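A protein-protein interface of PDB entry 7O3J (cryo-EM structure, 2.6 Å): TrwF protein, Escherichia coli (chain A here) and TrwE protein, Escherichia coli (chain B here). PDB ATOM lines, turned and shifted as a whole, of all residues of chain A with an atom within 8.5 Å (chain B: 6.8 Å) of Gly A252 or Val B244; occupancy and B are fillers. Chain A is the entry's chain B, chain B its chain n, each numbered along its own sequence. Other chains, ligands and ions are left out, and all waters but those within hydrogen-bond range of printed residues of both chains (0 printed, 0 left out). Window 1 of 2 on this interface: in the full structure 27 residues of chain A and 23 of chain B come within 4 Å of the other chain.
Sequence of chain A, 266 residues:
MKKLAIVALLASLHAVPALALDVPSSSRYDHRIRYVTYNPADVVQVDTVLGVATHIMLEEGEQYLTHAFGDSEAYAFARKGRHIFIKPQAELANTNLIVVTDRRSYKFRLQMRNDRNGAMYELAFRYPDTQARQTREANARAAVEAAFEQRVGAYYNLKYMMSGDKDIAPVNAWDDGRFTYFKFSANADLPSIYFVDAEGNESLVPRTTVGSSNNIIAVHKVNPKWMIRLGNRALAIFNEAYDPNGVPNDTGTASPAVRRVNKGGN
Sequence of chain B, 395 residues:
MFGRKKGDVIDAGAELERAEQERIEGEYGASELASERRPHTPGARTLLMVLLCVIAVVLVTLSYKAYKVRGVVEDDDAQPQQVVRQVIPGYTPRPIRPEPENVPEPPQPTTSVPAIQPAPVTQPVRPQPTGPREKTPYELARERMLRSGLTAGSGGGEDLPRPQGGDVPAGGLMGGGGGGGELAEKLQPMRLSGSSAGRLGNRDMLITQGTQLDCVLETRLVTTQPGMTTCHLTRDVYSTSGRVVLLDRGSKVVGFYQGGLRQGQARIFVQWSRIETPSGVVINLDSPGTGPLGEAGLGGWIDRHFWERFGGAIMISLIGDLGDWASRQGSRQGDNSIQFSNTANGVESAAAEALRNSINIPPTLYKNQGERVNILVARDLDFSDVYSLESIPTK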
ATOM      1  N   VAL A 144      -6.123  29.719   8.284  1.00  0.00           N
ATOM      2  CA  VAL A 144      -6.663  28.363   8.267  1.00  0.00           C
ATOM      3  C   VAL A 144      -7.818  28.252   7.281  1.00  0.00           C
ATOM      4  O   VAL A 144      -7.905  27.288   6.515  1.00  0.00           O
ATOM      5  CB  VAL A 144      -7.080  27.934   9.685  1.00  0.00           C
ATOM      6  CG1 VAL A 144      -7.738  26.583   9.653  1.00  0.00           C
ATOM      7  CG2 VAL A 144      -5.871  27.878  10.586  1.00  0.00           C
ATOM      8  N   PHE A 148      -7.924  25.950   3.936  1.00  0.00           N
ATOM      9  CA  PHE A 148      -8.985  24.984   3.679  1.00  0.00           C
ATOM     10  C   PHE A 148      -9.641  25.234   2.328  1.00  0.00           C
ATOM     11  O   PHE A 148      -9.950  24.288   1.596  1.00  0.00           O
ATOM     12  CB  PHE A 148     -10.027  25.034   4.792  1.00  0.00           C
ATOM     13  CG  PHE A 148      -9.712  24.143   5.953  1.00  0.00           C
ATOM     14  CD1 PHE A 148      -9.400  22.816   5.758  1.00  0.00           C
ATOM     15  CD2 PHE A 148      -9.739  24.632   7.240  1.00  0.00           C
ATOM     16  CE1 PHE A 148      -9.113  22.001   6.821  1.00  0.00           C
ATOM     17  CE2 PHE A 148      -9.454  23.816   8.306  1.00  0.00           C
ATOM     18  CZ  PHE A 148      -9.142  22.503   8.096  1.00  0.00           C
ATOM     19  N   ARG A 178      -9.529  11.153  -0.780  1.00  0.00           N
ATOM     20  CA  ARG A 178      -9.832  11.023   0.636  1.00  0.00           C
ATOM     21  C   ARG A 178     -11.317  10.854   0.896  1.00  0.00           C
ATOM     22  O   ARG A 178     -11.709   9.973   1.665  1.00  0.00           O
ATOM     23  CB  ARG A 178      -9.295  12.239   1.400  1.00  0.00           C
ATOM     24  CG  ARG A 178      -9.610  12.227   2.879  1.00  0.00           C
ATOM     25  CD  ARG A 178      -8.473  12.807   3.683  1.00  0.00           C
ATOM     26  NE  ARG A 178      -7.188  12.292   3.233  1.00  0.00           N
ATOM     27  CZ  ARG A 178      -6.061  12.991   3.246  1.00  0.00           C
ATOM     28  NH1 ARG A 178      -6.056  14.237   3.688  1.00  0.00           N
ATOM     29  NH2 ARG A 178      -4.937  12.441   2.812  1.00  0.00           N
ATOM     30  N   PHE A 179     -12.158  11.675   0.277  1.00  0.00           N
ATOM     31  CA  PHE A 179     -13.601  11.606   0.433  1.00  0.00           C
ATOM     32  C   PHE A 179     -14.238  11.271  -0.905  1.00  0.00           C
ATOM     33  O   PHE A 179     -13.671  11.555  -1.959  1.00  0.00           O
ATOM     34  CB  PHE A 179     -14.181  12.929   0.937  1.00  0.00           C
ATOM     35  CG  PHE A 179     -13.908  13.216   2.379  1.00  0.00           C
ATOM     36  CD1 PHE A 179     -13.160  12.356   3.150  1.00  0.00           C
ATOM     37  CD2 PHE A 179     -14.412  14.354   2.966  1.00  0.00           C
ATOM     38  CE1 PHE A 179     -12.918  12.630   4.472  1.00  0.00           C
ATOM     39  CE2 PHE A 179     -14.171  14.627   4.290  1.00  0.00           C
ATOM     40  CZ  PHE A 179     -13.425  13.765   5.039  1.00  0.00           C
ATOM     41  N   HIS A 220     -16.769   9.866   4.185  1.00  0.00           N
ATOM     42  CA  HIS A 220     -15.414  10.045   4.682  1.00  0.00           C
ATOM     43  C   HIS A 220     -14.517   8.864   4.372  1.00  0.00           C
ATOM     44  O   HIS A 220     -13.599   8.570   5.143  1.00  0.00           O
ATOM     45  CB  HIS A 220     -15.444  10.303   6.187  1.00  0.00           C
ATOM     46  CG  HIS A 220     -16.169  11.552   6.573  1.00  0.00           C
ATOM     47  ND1 HIS A 220     -16.411  12.575   5.685  1.00  0.00           N
ATOM     48  CD2 HIS A 220     -16.701  11.944   7.753  1.00  0.00           C
ATOM     49  CE1 HIS A 220     -17.063  13.543   6.300  1.00  0.00           C
ATOM     50  NE2 HIS A 220     -17.250  13.186   7.557  1.00  0.00           N
ATOM     51  N   PRO A 248      -1.606   9.412   2.004  1.00  0.00           N
ATOM     52  CA  PRO A 248      -1.568   9.404   3.469  1.00  0.00           C
ATOM     53  C   PRO A 248      -1.982  10.736   4.069  1.00  0.00           C
ATOM     54  O   PRO A 248      -1.805  11.800   3.476  1.00  0.00           O
ATOM     55  CB  PRO A 248      -0.101   9.089   3.784  1.00  0.00           C
ATOM     56  CG  PRO A 248       0.639   9.425   2.545  1.00  0.00           C
ATOM     57  CD  PRO A 248      -0.288   9.135   1.418  1.00  0.00           C
ATOM     58  N   ASN A 249      -2.541  10.659   5.275  1.00  0.00           N
ATOM     59  CA  ASN A 249      -3.013  11.831   6.007  1.00  0.00           C
ATOM     60  C   ASN A 249      -1.998  12.153   7.097  1.00  0.00           C
ATOM     61  O   ASN A 249      -2.128  11.749   8.250  1.00  0.00           O
ATOM     62  CB  ASN A 249      -4.396  11.570   6.583  1.00  0.00           C
ATOM     63  CG  ASN A 249      -5.042  12.814   7.139  1.00  0.00           C
ATOM     64  OD1 ASN A 249      -4.407  13.855   7.260  1.00  0.00           O
ATOM     65  ND2 ASN A 249      -6.315  12.711   7.483  1.00  0.00           N
ATOM     66  N   ASP A 250      -0.975  12.910   6.719  1.00  0.00           N
ATOM     67  CA  ASP A 250       0.112  13.231   7.629  1.00  0.00           C
ATOM     68  C   ASP A 250      -0.170  14.439   8.507  1.00  0.00           C
ATOM     69  O   ASP A 250       0.590  14.688   9.445  1.00  0.00           O
ATOM     70  CB  ASP A 250       1.394  13.481   6.839  1.00  0.00           C
ATOM     71  CG  ASP A 250       1.924  12.231   6.179  1.00  0.00           C
ATOM     72  OD1 ASP A 250       1.627  12.019   4.987  1.00  0.00           O
ATOM     73  OD2 ASP A 250       2.637  11.459   6.847  1.00  0.00           O
ATOM     74  N   THR A 251      -1.238  15.190   8.236  1.00  0.00           N
ATOM     75  CA  THR A 251      -1.475  16.455   8.913  1.00  0.00           C
ATOM     76  C   THR A 251      -2.575  16.408   9.958  1.00  0.00           C
ATOM     77  O   THR A 251      -2.617  17.289  10.818  1.00  0.00           O
ATOM     78  CB  THR A 251      -1.822  17.545   7.893  1.00  0.00           C
ATOM     79  OG1 THR A 251      -2.806  17.049   6.983  1.00  0.00           O
ATOM     80  CG2 THR A 251      -0.590  17.949   7.120  1.00  0.00           C
ATOM     81  N   GLY A 252      -3.454  15.415   9.918  1.00  0.00           N
ATOM     82  CA  GLY A 252      -4.553  15.346  10.851  1.00  0.00           C
ATOM     83  C   GLY A 252      -5.773  16.140  10.454  1.00  0.00           C
ATOM     84  O   GLY A 252      -6.744  16.173  11.212  1.00  0.00           O
ATOM     85  N   THR A 253      -5.750  16.786   9.297  1.00  0.00           N
ATOM     86  CA  THR A 253      -6.877  17.537   8.781  1.00  0.00           C
ATOM     87  C   THR A 253      -7.244  17.008   7.405  1.00  0.00           C
ATOM     88  O   THR A 253      -6.546  16.175   6.828  1.00  0.00           O
ATOM     89  CB  THR A 253      -6.561  19.034   8.703  1.00  0.00           C
ATOM     90  OG1 THR A 253      -5.372  19.228   7.934  1.00  0.00           O
ATOM     91  CG2 THR A 253      -6.353  19.604  10.084  1.00  0.00           C
ATOM     92  N   ALA A 254      -8.361  17.500   6.880  1.00  0.00           N
ATOM     93  CA  ALA A 254      -8.778  17.138   5.535  1.00  0.00           C
ATOM     94  C   ALA A 254      -7.966  17.842   4.460  1.00  0.00           C
ATOM     95  O   ALA A 254      -8.123  17.521   3.280  1.00  0.00           O
ATOM     96  CB  ALA A 254     -10.259  17.451   5.339  1.00  0.00           C
ATOM     97  N   SER A 255      -7.109  18.784   4.837  1.00  0.00           N
ATOM     98  CA  SER A 255      -6.303  19.512   3.883  1.00  0.00           C
ATOM     99  C   SER A 255      -4.824  19.269   4.142  1.00  0.00           C
ATOM    100  O   SER A 255      -4.415  19.128   5.297  1.00  0.00           O
ATOM    101  CB  SER A 255      -6.591  21.014   3.961  1.00  0.00           C
ATOM    102  OG  SER A 255      -5.667  21.747   3.183  1.00  0.00           O
ATOM    103  N   PRO A 256      -4.002  19.210   3.094  1.00  0.00           N
ATOM    104  CA  PRO A 256      -2.552  19.111   3.291  1.00  0.00           C
ATOM    105  C   PRO A 256      -1.888  20.424   3.661  1.00  0.00           C
ATOM    106  O   PRO A 256      -0.655  20.475   3.720  1.00  0.00           O
ATOM    107  CB  PRO A 256      -2.050  18.618   1.924  1.00  0.00           C
ATOM    108  CG  PRO A 256      -3.265  18.207   1.165  1.00  0.00           C
ATOM    109  CD  PRO A 256      -4.371  19.043   1.683  1.00  0.00           C
ATOM    110  N   VAL A 258      -2.943  22.401   6.472  1.00  0.00           N
ATOM    111  CA  VAL A 258      -3.212  22.723   7.869  1.00  0.00           C
ATOM    112  C   VAL A 258      -2.711  21.578   8.735  1.00  0.00           C
ATOM    113  O   VAL A 258      -3.130  20.433   8.542  1.00  0.00           O
ATOM    114  CB  VAL A 258      -4.722  22.955   8.092  1.00  0.00           C
ATOM    115  CG1 VAL A 258      -5.000  23.478   9.485  1.00  0.00           C
ATOM    116  CG2 VAL A 258      -5.295  23.887   7.046  1.00  0.00           C
ATOM    117  N   ARG A 259      -1.823  21.863   9.696  1.00  0.00           N
ATOM    118  CA  ARG A 259      -1.552  20.868  10.725  1.00  0.00           C
ATOM    119  C   ARG A 259      -2.643  20.919  11.778  1.00  0.00           C
ATOM    120  O   ARG A 259      -3.217  21.973  12.047  1.00  0.00           O
ATOM    121  CB  ARG A 259      -0.213  20.987  11.513  1.00  0.00           C
ATOM    122  CG  ARG A 259       1.093  20.489  10.893  1.00  0.00           C
ATOM    123  CD  ARG A 259       1.847  21.408   9.951  1.00  0.00           C
ATOM    124  NE  ARG A 259       2.322  22.566  10.713  1.00  0.00           N
ATOM    125  CZ  ARG A 259       2.816  23.686  10.194  1.00  0.00           C
ATOM    126  NH1 ARG A 259       3.206  24.668  10.995  1.00  0.00           N
ATOM    127  NH2 ARG A 259       2.992  23.804   8.891  1.00  0.00           N
ATOM    128  N   ARG A 260      -2.907  19.766  12.373  1.00  0.00           N
ATOM    129  CA  ARG A 260      -3.547  19.685  13.674  1.00  0.00           C
ATOM    130  C   ARG A 260      -2.450  19.487  14.708  1.00  0.00           C
ATOM    131  O   ARG A 260      -1.696  18.513  14.634  1.00  0.00           O
ATOM    132  CB  ARG A 260      -4.540  18.530  13.713  1.00  0.00           C
ATOM    133  CG  ARG A 260      -5.381  18.472  14.953  1.00  0.00           C
ATOM    134  CD  ARG A 260      -5.872  17.071  15.166  1.00  0.00           C
ATOM    135  NE  ARG A 260      -4.771  16.123  15.146  1.00  0.00           N
ATOM    136  CZ  ARG A 260      -4.922  14.807  15.193  1.00  0.00           C
ATOM    137  NH1 ARG A 260      -3.867  14.012  15.168  1.00  0.00           N
ATOM    138  NH2 ARG A 260      -6.132  14.287  15.264  1.00  0.00           N
ATOM    139  N   VAL A 261      -2.341  20.409  15.657  1.00  0.00           N
ATOM    140  CA  VAL A 261      -1.249  20.384  16.618  1.00  0.00           C
ATOM    141  C   VAL A 261      -1.811  20.169  18.014  1.00  0.00           C
ATOM    142  O   VAL A 261      -2.942  20.556  18.321  1.00  0.00           O
ATOM    143  CB  VAL A 261      -0.392  21.668  16.552  1.00  0.00           C
ATOM    144  CG1 VAL A 261       0.409  21.688  15.274  1.00  0.00           C
ATOM    145  CG2 VAL A 261      -1.258  22.886  16.618  1.00  0.00           C
ATOM    146  N   ARG B 203     -17.370  23.801  15.158  1.00  0.00           N
ATOM    147  CA  ARG B 203     -17.666  22.553  14.481  1.00  0.00           C
ATOM    148  C   ARG B 203     -16.424  21.864  13.946  1.00  0.00           C
ATOM    149  O   ARG B 203     -16.543  20.798  13.341  1.00  0.00           O
ATOM    150  CB  ARG B 203     -18.661  22.799  13.352  1.00  0.00           C
ATOM    151  CG  ARG B 203     -20.047  23.106  13.857  1.00  0.00           C
ATOM    152  CD  ARG B 203     -20.963  23.529  12.745  1.00  0.00           C
ATOM    153  NE  ARG B 203     -21.092  22.512  11.713  1.00  0.00           N
ATOM    154  CZ  ARG B 203     -20.671  22.664  10.467  1.00  0.00           C
ATOM    155  NH1 ARG B 203     -20.091  23.795  10.100  1.00  0.00           N
ATOM    156  NH2 ARG B 203     -20.832  21.691   9.588  1.00  0.00           N
ATOM    157  N   ASP B 204     -15.245  22.445  14.142  1.00  0.00           N
ATOM    158  CA  ASP B 204     -14.000  21.772  13.811  1.00  0.00           C
ATOM    159  C   ASP B 204     -13.439  20.962  14.963  1.00  0.00           C
ATOM    160  O   ASP B 204     -12.651  20.046  14.727  1.00  0.00           O
ATOM    161  CB  ASP B 204     -12.945  22.781  13.357  1.00  0.00           C
ATOM    162  CG  ASP B 204     -13.209  23.303  11.972  1.00  0.00           C
ATOM    163  OD1 ASP B 204     -13.650  22.509  11.120  1.00  0.00           O
ATOM    164  OD2 ASP B 204     -12.961  24.499  11.727  1.00  0.00           O
ATOM    165  N   MET B 205     -13.822  21.277  16.191  1.00  0.00           N
ATOM    166  CA  MET B 205     -13.390  20.542  17.368  1.00  0.00           C
ATOM    167  C   MET B 205     -14.554  19.803  18.007  1.00  0.00           C
ATOM    168  O   MET B 205     -14.651  19.728  19.229  1.00  0.00           O
ATOM    169  CB  MET B 205     -12.737  21.484  18.378  1.00  0.00           C
ATOM    170  CG  MET B 205     -11.388  22.036  17.962  1.00  0.00           C
ATOM    171  SD  MET B 205     -10.361  20.833  17.114  1.00  0.00           S
ATOM    172  CE  MET B 205      -9.416  21.892  16.034  1.00  0.00           C
ATOM    173  N   LEU B 206     -15.444  19.248  17.193  1.00  0.00           N
ATOM    174  CA  LEU B 206     -16.699  18.711  17.687  1.00  0.00           C
ATOM    175  C   LEU B 206     -17.049  17.418  16.975  1.00  0.00           C
ATOM    176  O   LEU B 206     -16.876  17.298  15.763  1.00  0.00           O
ATOM    177  CB  LEU B 206     -17.825  19.723  17.490  1.00  0.00           C
ATOM    178  CG  LEU B 206     -18.990  19.765  18.468  1.00  0.00           C
ATOM    179  CD1 LEU B 206     -18.515  19.675  19.894  1.00  0.00           C
ATOM    180  CD2 LEU B 206     -19.746  21.046  18.246  1.00  0.00           C
ATOM    181  N   VAL B 237     -11.872   9.413  12.370  1.00  0.00           N
ATOM    182  CA  VAL B 237     -13.145  10.067  12.631  1.00  0.00           C
ATOM    183  C   VAL B 237     -12.925  11.565  12.509  1.00  0.00           C
ATOM    184  O   VAL B 237     -12.087  12.134  13.214  1.00  0.00           O
ATOM    185  CB  VAL B 237     -13.701   9.698  14.012  1.00  0.00           C
ATOM    186  CG1 VAL B 237     -15.054  10.314  14.213  1.00  0.00           C
ATOM    187  CG2 VAL B 237     -13.793   8.203  14.145  1.00  0.00           C
ATOM    188  N   TYR B 238     -13.670  12.201  11.619  1.00  0.00           N
ATOM    189  CA  TYR B 238     -13.531  13.621  11.365  1.00  0.00           C
ATOM    190  C   TYR B 238     -14.502  14.410  12.231  1.00  0.00           C
ATOM    191  O   TYR B 238     -15.338  13.857  12.945  1.00  0.00           O
ATOM    192  CB  TYR B 238     -13.749  13.915   9.885  1.00  0.00           C
ATOM    193  CG  TYR B 238     -12.600  13.484   9.028  1.00  0.00           C
ATOM    194  CD1 TYR B 238     -12.398  12.153   8.732  1.00  0.00           C
ATOM    195  CD2 TYR B 238     -11.709  14.406   8.523  1.00  0.00           C
ATOM    196  CE1 TYR B 238     -11.350  11.755   7.959  1.00  0.00           C
ATOM    197  CE2 TYR B 238     -10.658  14.018   7.746  1.00  0.00           C
ATOM    198  CZ  TYR B 238     -10.480  12.691   7.467  1.00  0.00           C
ATOM    199  OH  TYR B 238      -9.427  12.291   6.688  1.00  0.00           O
ATOM    200  N   SER B 239     -14.379  15.728  12.175  1.00  0.00           N
ATOM    201  CA  SER B 239     -15.282  16.602  12.897  1.00  0.00           C
ATOM    202  C   SER B 239     -16.600  16.731  12.142  1.00  0.00           C
ATOM    203  O   SER B 239     -16.757  16.247  11.021  1.00  0.00           O
ATOM    204  CB  SER B 239     -14.641  17.965  13.098  1.00  0.00           C
ATOM    205  OG  SER B 239     -14.007  18.393  11.911  1.00  0.00           O
ATOM    206  N   THR B 240     -17.568  17.393  12.776  1.00  0.00           N
ATOM    207  CA  THR B 240     -18.849  17.604  12.117  1.00  0.00           C
ATOM    208  C   THR B 240     -18.701  18.466  10.877  1.00  0.00           C
ATOM    209  O   THR B 240     -19.432  18.277   9.901  1.00  0.00           O
ATOM    210  CB  THR B 240     -19.847  18.235  13.076  1.00  0.00           C
ATOM    211  OG1 THR B 240     -19.233  19.332  13.753  1.00  0.00           O
ATOM    212  CG2 THR B 240     -20.259  17.226  14.087  1.00  0.00           C
ATOM    213  N   SER B 241     -17.772  19.416  10.892  1.00  0.00           N
ATOM    214  CA  SER B 241     -17.453  20.138   9.673  1.00  0.00           C
ATOM    215  C   SER B 241     -16.759  19.252   8.651  1.00  0.00           C
ATOM    216  O   SER B 241     -16.729  19.600   7.469  1.00  0.00           O
ATOM    217  CB  SER B 241     -16.583  21.348   9.993  1.00  0.00           C
ATOM    218  OG  SER B 241     -15.406  20.962  10.670  1.00  0.00           O
ATOM    219  N   GLY B 242     -16.211  18.119   9.077  1.00  0.00           N
ATOM    220  CA  GLY B 242     -15.537  17.221   8.165  1.00  0.00           C
ATOM    221  C   GLY B 242     -14.182  17.690   7.698  1.00  0.00           C
ATOM    222  O   GLY B 242     -13.803  17.414   6.560  1.00  0.00           O
ATOM    223  N   ARG B 243     -13.433  18.393   8.546  1.00  0.00           N
ATOM    224  CA  ARG B 243     -12.161  18.967   8.139  1.00  0.00           C
ATOM    225  C   ARG B 243     -10.987  18.603   9.031  1.00  0.00           C
ATOM    226  O   ARG B 243      -9.847  18.731   8.587  1.00  0.00           O
ATOM    227  CB  ARG B 243     -12.263  20.498   8.072  1.00  0.00           C
ATOM    228  CG  ARG B 243     -13.406  20.991   7.214  1.00  0.00           C
ATOM    229  CD  ARG B 243     -13.317  22.469   6.952  1.00  0.00           C
ATOM    230  NE  ARG B 243     -13.307  23.239   8.185  1.00  0.00           N
ATOM    231  CZ  ARG B 243     -13.291  24.565   8.229  1.00  0.00           C
ATOM    232  NH1 ARG B 243     -13.278  25.192   9.395  1.00  0.00           N
ATOM    233  NH2 ARG B 243     -13.285  25.262   7.105  1.00  0.00           N
ATOM    234  N   VAL B 244     -11.224  18.155  10.257  1.00  0.00           N
ATOM    235  CA  VAL B 244     -10.165  17.836  11.204  1.00  0.00           C
ATOM    236  C   VAL B 244     -10.368  16.409  11.683  1.00  0.00           C
ATOM    237  O   VAL B 244     -11.488  16.025  12.028  1.00  0.00           O
ATOM    238  CB  VAL B 244     -10.160  18.809  12.397  1.00  0.00           C
ATOM    239  CG1 VAL B 244      -9.030  18.494  13.334  1.00  0.00           C
ATOM    240  CG2 VAL B 244     -10.057  20.225  11.908  1.00  0.00           C
ATOM    241  N   VAL B 245      -9.294  15.625  11.700  1.00  0.00           N
ATOM    242  CA  VAL B 245      -9.341  14.272  12.239  1.00  0.00           C
ATOM    243  C   VAL B 245      -9.263  14.371  13.757  1.00  0.00           C
ATOM    244  O   VAL B 245      -8.223  14.720  14.312  1.00  0.00           O
ATOM    245  CB  VAL B 245      -8.209  13.403  11.690  1.00  0.00           C
ATOM    246  CG1 VAL B 245      -8.292  12.027  12.275  1.00  0.00           C
ATOM    247  CG2 VAL B 245      -8.273  13.341  10.196  1.00  0.00           C
ATOM    248  N   LEU B 246     -10.358  14.052  14.431  1.00  0.00           N
ATOM    249  CA  LEU B 246     -10.413  14.166  15.881  1.00  0.00           C
ATOM    250  C   LEU B 246     -10.044  12.876  16.593  1.00  0.00           C
ATOM    251  O   LEU B 246      -9.405  12.922  17.643  1.00  0.00           O
ATOM    252  CB  LEU B 246     -11.807  14.615  16.312  1.00  0.00           C
ATOM    253  CG  LEU B 246     -12.154  16.039  15.890  1.00  0.00           C
ATOM    254  CD1 LEU B 246     -13.476  16.425  16.463  1.00  0.00           C
ATOM    255  CD2 LEU B 246     -11.088  17.002  16.332  1.00  0.00           C
ATOM    256  N   LEU B 247     -10.429  11.728  16.050  1.00  0.00           N
ATOM    257  CA  LEU B 247     -10.040  10.430  16.583  1.00  0.00           C
ATOM    258  C   LEU B 247      -9.292   9.680  15.497  1.00  0.00           C
ATOM    259  O   LEU B 247      -9.859   9.386  14.443  1.00  0.00           O
ATOM    260  CB  LEU B 247     -11.259   9.637  17.043  1.00  0.00           C
ATOM    261  CG  LEU B 247     -12.026  10.241  18.209  1.00  0.00           C
ATOM    262  CD1 LEU B 247     -13.324   9.515  18.412  1.00  0.00           C
ATOM    263  CD2 LEU B 247     -11.193  10.177  19.455  1.00  0.00           C
ATOM    264  N   ASP B 248      -8.030   9.370  15.751  1.00  0.00           N
ATOM    265  CA  ASP B 248      -7.214   8.698  14.759  1.00  0.00           C
ATOM    266  C   ASP B 248      -7.581   7.224  14.669  1.00  0.00           C
ATOM    267  O   ASP B 248      -8.150   6.642  15.591  1.00  0.00           O
ATOM    268  CB  ASP B 248      -5.740   8.839  15.104  1.00  0.00           C
ATOM    269  CG  ASP B 248      -5.364  10.256  15.437  1.00  0.00           C
ATOM    270  OD1 ASP B 248      -4.644  10.463  16.435  1.00  0.00           O
ATOM    271  OD2 ASP B 248      -5.787  11.168  14.702  1.00  0.00           O
ATOM    272  N   TYR B 387      -6.603  20.147  20.853  1.00  0.00           N
ATOM    273  CA  TYR B 387      -6.113  20.368  19.504  1.00  0.00           C
ATOM    274  C   TYR B 387      -6.220  21.839  19.148  1.00  0.00           C
ATOM    275  O   TYR B 387      -7.013  22.582  19.725  1.00  0.00           O
ATOM    276  CB  TYR B 387      -6.891  19.572  18.456  1.00  0.00           C
ATOM    277  CG  TYR B 387      -6.804  18.080  18.585  1.00  0.00           C
ATOM    278  CD1 TYR B 387      -5.584  17.442  18.663  1.00  0.00           C
ATOM    279  CD2 TYR B 387      -7.950  17.308  18.610  1.00  0.00           C
ATOM    280  CE1 TYR B 387      -5.512  16.082  18.775  1.00  0.00           C
ATOM    281  CE2 TYR B 387      -7.883  15.955  18.722  1.00  0.00           C
ATOM    282  CZ  TYR B 387      -6.665  15.346  18.804  1.00  0.00           C
ATOM    283  OH  TYR B 387      -6.604  13.982  18.912  1.00  0.00           O
ATOM    284  N   SER B 388      -5.409  22.242  18.179  1.00  0.00           N
ATOM    285  CA  SER B 388      -5.539  23.539  17.542  1.00  0.00           C
ATOM    286  C   SER B 388      -5.025  23.408  16.119  1.00  0.00           C
ATOM    287  O   SER B 388      -4.313  22.462  15.789  1.00  0.00           O
ATOM    288  CB  SER B 388      -4.789  24.630  18.309  1.00  0.00           C
ATOM    289  OG  SER B 388      -3.392  24.438  18.242  1.00  0.00           O
ATOM    290  N   LEU B 389      -5.407  24.355  15.276  1.00  0.00           N
ATOM    291  CA  LEU B 389      -5.080  24.309  13.860  1.00  0.00           C
ATOM    292  C   LEU B 389      -4.089  25.409  13.512  1.00  0.00           C
ATOM    293  O   LEU B 389      -4.154  26.509  14.063  1.00  0.00           O
ATOM    294  CB  LEU B 389      -6.333  24.462  13.001  1.00  0.00           C
ATOM    295  CG  LEU B 389      -7.464  23.478  13.269  1.00  0.00           C
ATOM    296  CD1 LEU B 389      -8.725  23.951  12.597  1.00  0.00           C
ATOM    297  CD2 LEU B 389      -7.079  22.111  12.772  1.00  0.00           C
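The side-chain hydroxyl (OH) of Tyr B238 is in hydrogen-bond range of the side-chain amide nitrogen (ND2) of Asn A249 (3.2 Å). N of Ala A254 lies within hydrogen-bond range of O of Arg B243, at 2.6 Å. The backbone NH of Val B245 is in hydrogen-bond range of the backbone carbonyl oxygen of Gly A252, 2.7 Å away. The guanidinium group (NH2) of Arg A260 lies within salt-bridge range of the side-chain carboxylate (OD2) of Asp B248 (3.2 Å). The backbone NH (N) of Val A261 is in hydrogen-bond range of the backbone carbonyl oxygen (O) of Ser B388 (2.8 Å). The guanidinium group (NH2) of Arg A260 lies close to the backbone carbonyl oxygen (O) of Val B245, at 2.3 Å.
The side-chain carboxylate of Asp B204 is in salt-bridge range of the guanidinium group of Arg B243 (2.5 Å). The side-chain amide oxygen of Asn A249 lies within hydrogen-bond range of the backbone NH of Gly A252. OD1 of Asn A249 lies close to O of Thr A253, at 3.2 Å. O of Ser A255 sits at hydrogen-bond distance from OG1 of Thr A253.
Phe A148 touches Arg B243 (CD2 to NH2, 3.6 Å). CE1 of Phe A179 touches CZ of Tyr B238 (3.9 Å). ND2 of Asn A249 touches CG2 of Val B245, at 3.4 Å. Val B244 touches Gly A252 (C to O, 3.7 Å). CA of Thr A253 touches O of Arg B243 (3.2 Å). Leu B389 touches Thr A253. Ala A254 touches Gly B242. Val A258 touches Leu B389. Arg A260 touches Val B244.
Asp A250 touches none of the printed residues of chain B. Gly A252 touches two residues of chain B. Printed residues of chain B within 4 Å of Thr A253: Arg B243 and Leu B389. Asp B204 touches none of the printed residues of chain A. Of the printed residues of chain A, Val B245 touches Asn A249 (3.4 Å), Gly A252 (2.7 Å) and Arg A260 (2.3 Å). The nearest residue of chain A that does not touch Val B244 is Thr A253 (4.1 Å). The nearest printed residue of chain B that does not touch Phe A148 is Leu B389 (4.4 Å).
Of the 19 printed residues of chain B, 9 touch a printed residue of chain A. Hydrophobic or aromatic side chains of chain B that line the printed part of chain A: Tyr B238, Val B244, Val B245, Tyr B387 and Leu B389. Printed residues of chain A that touch a printed residue of chain B: Phe A148, Arg A178, Phe A179, Asn A249, Gly A252, Thr A253, Ala A254, Val A258, Arg A259, Arg A260 and Val A261. Hydrophobic or aromatic side chains of chain A that line the printed part of chain B: Phe A148, Phe A179, Ala A254, Val A258 and Val A261. Among the printed residues, 22 pairs touch across the chains. Among the printed residues, Asp or Glu carboxylates within 4 Å of a Lys or Arg side-chain nitrogen of the other chain: Arg A260 with Asp B248 (3.2 Å).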
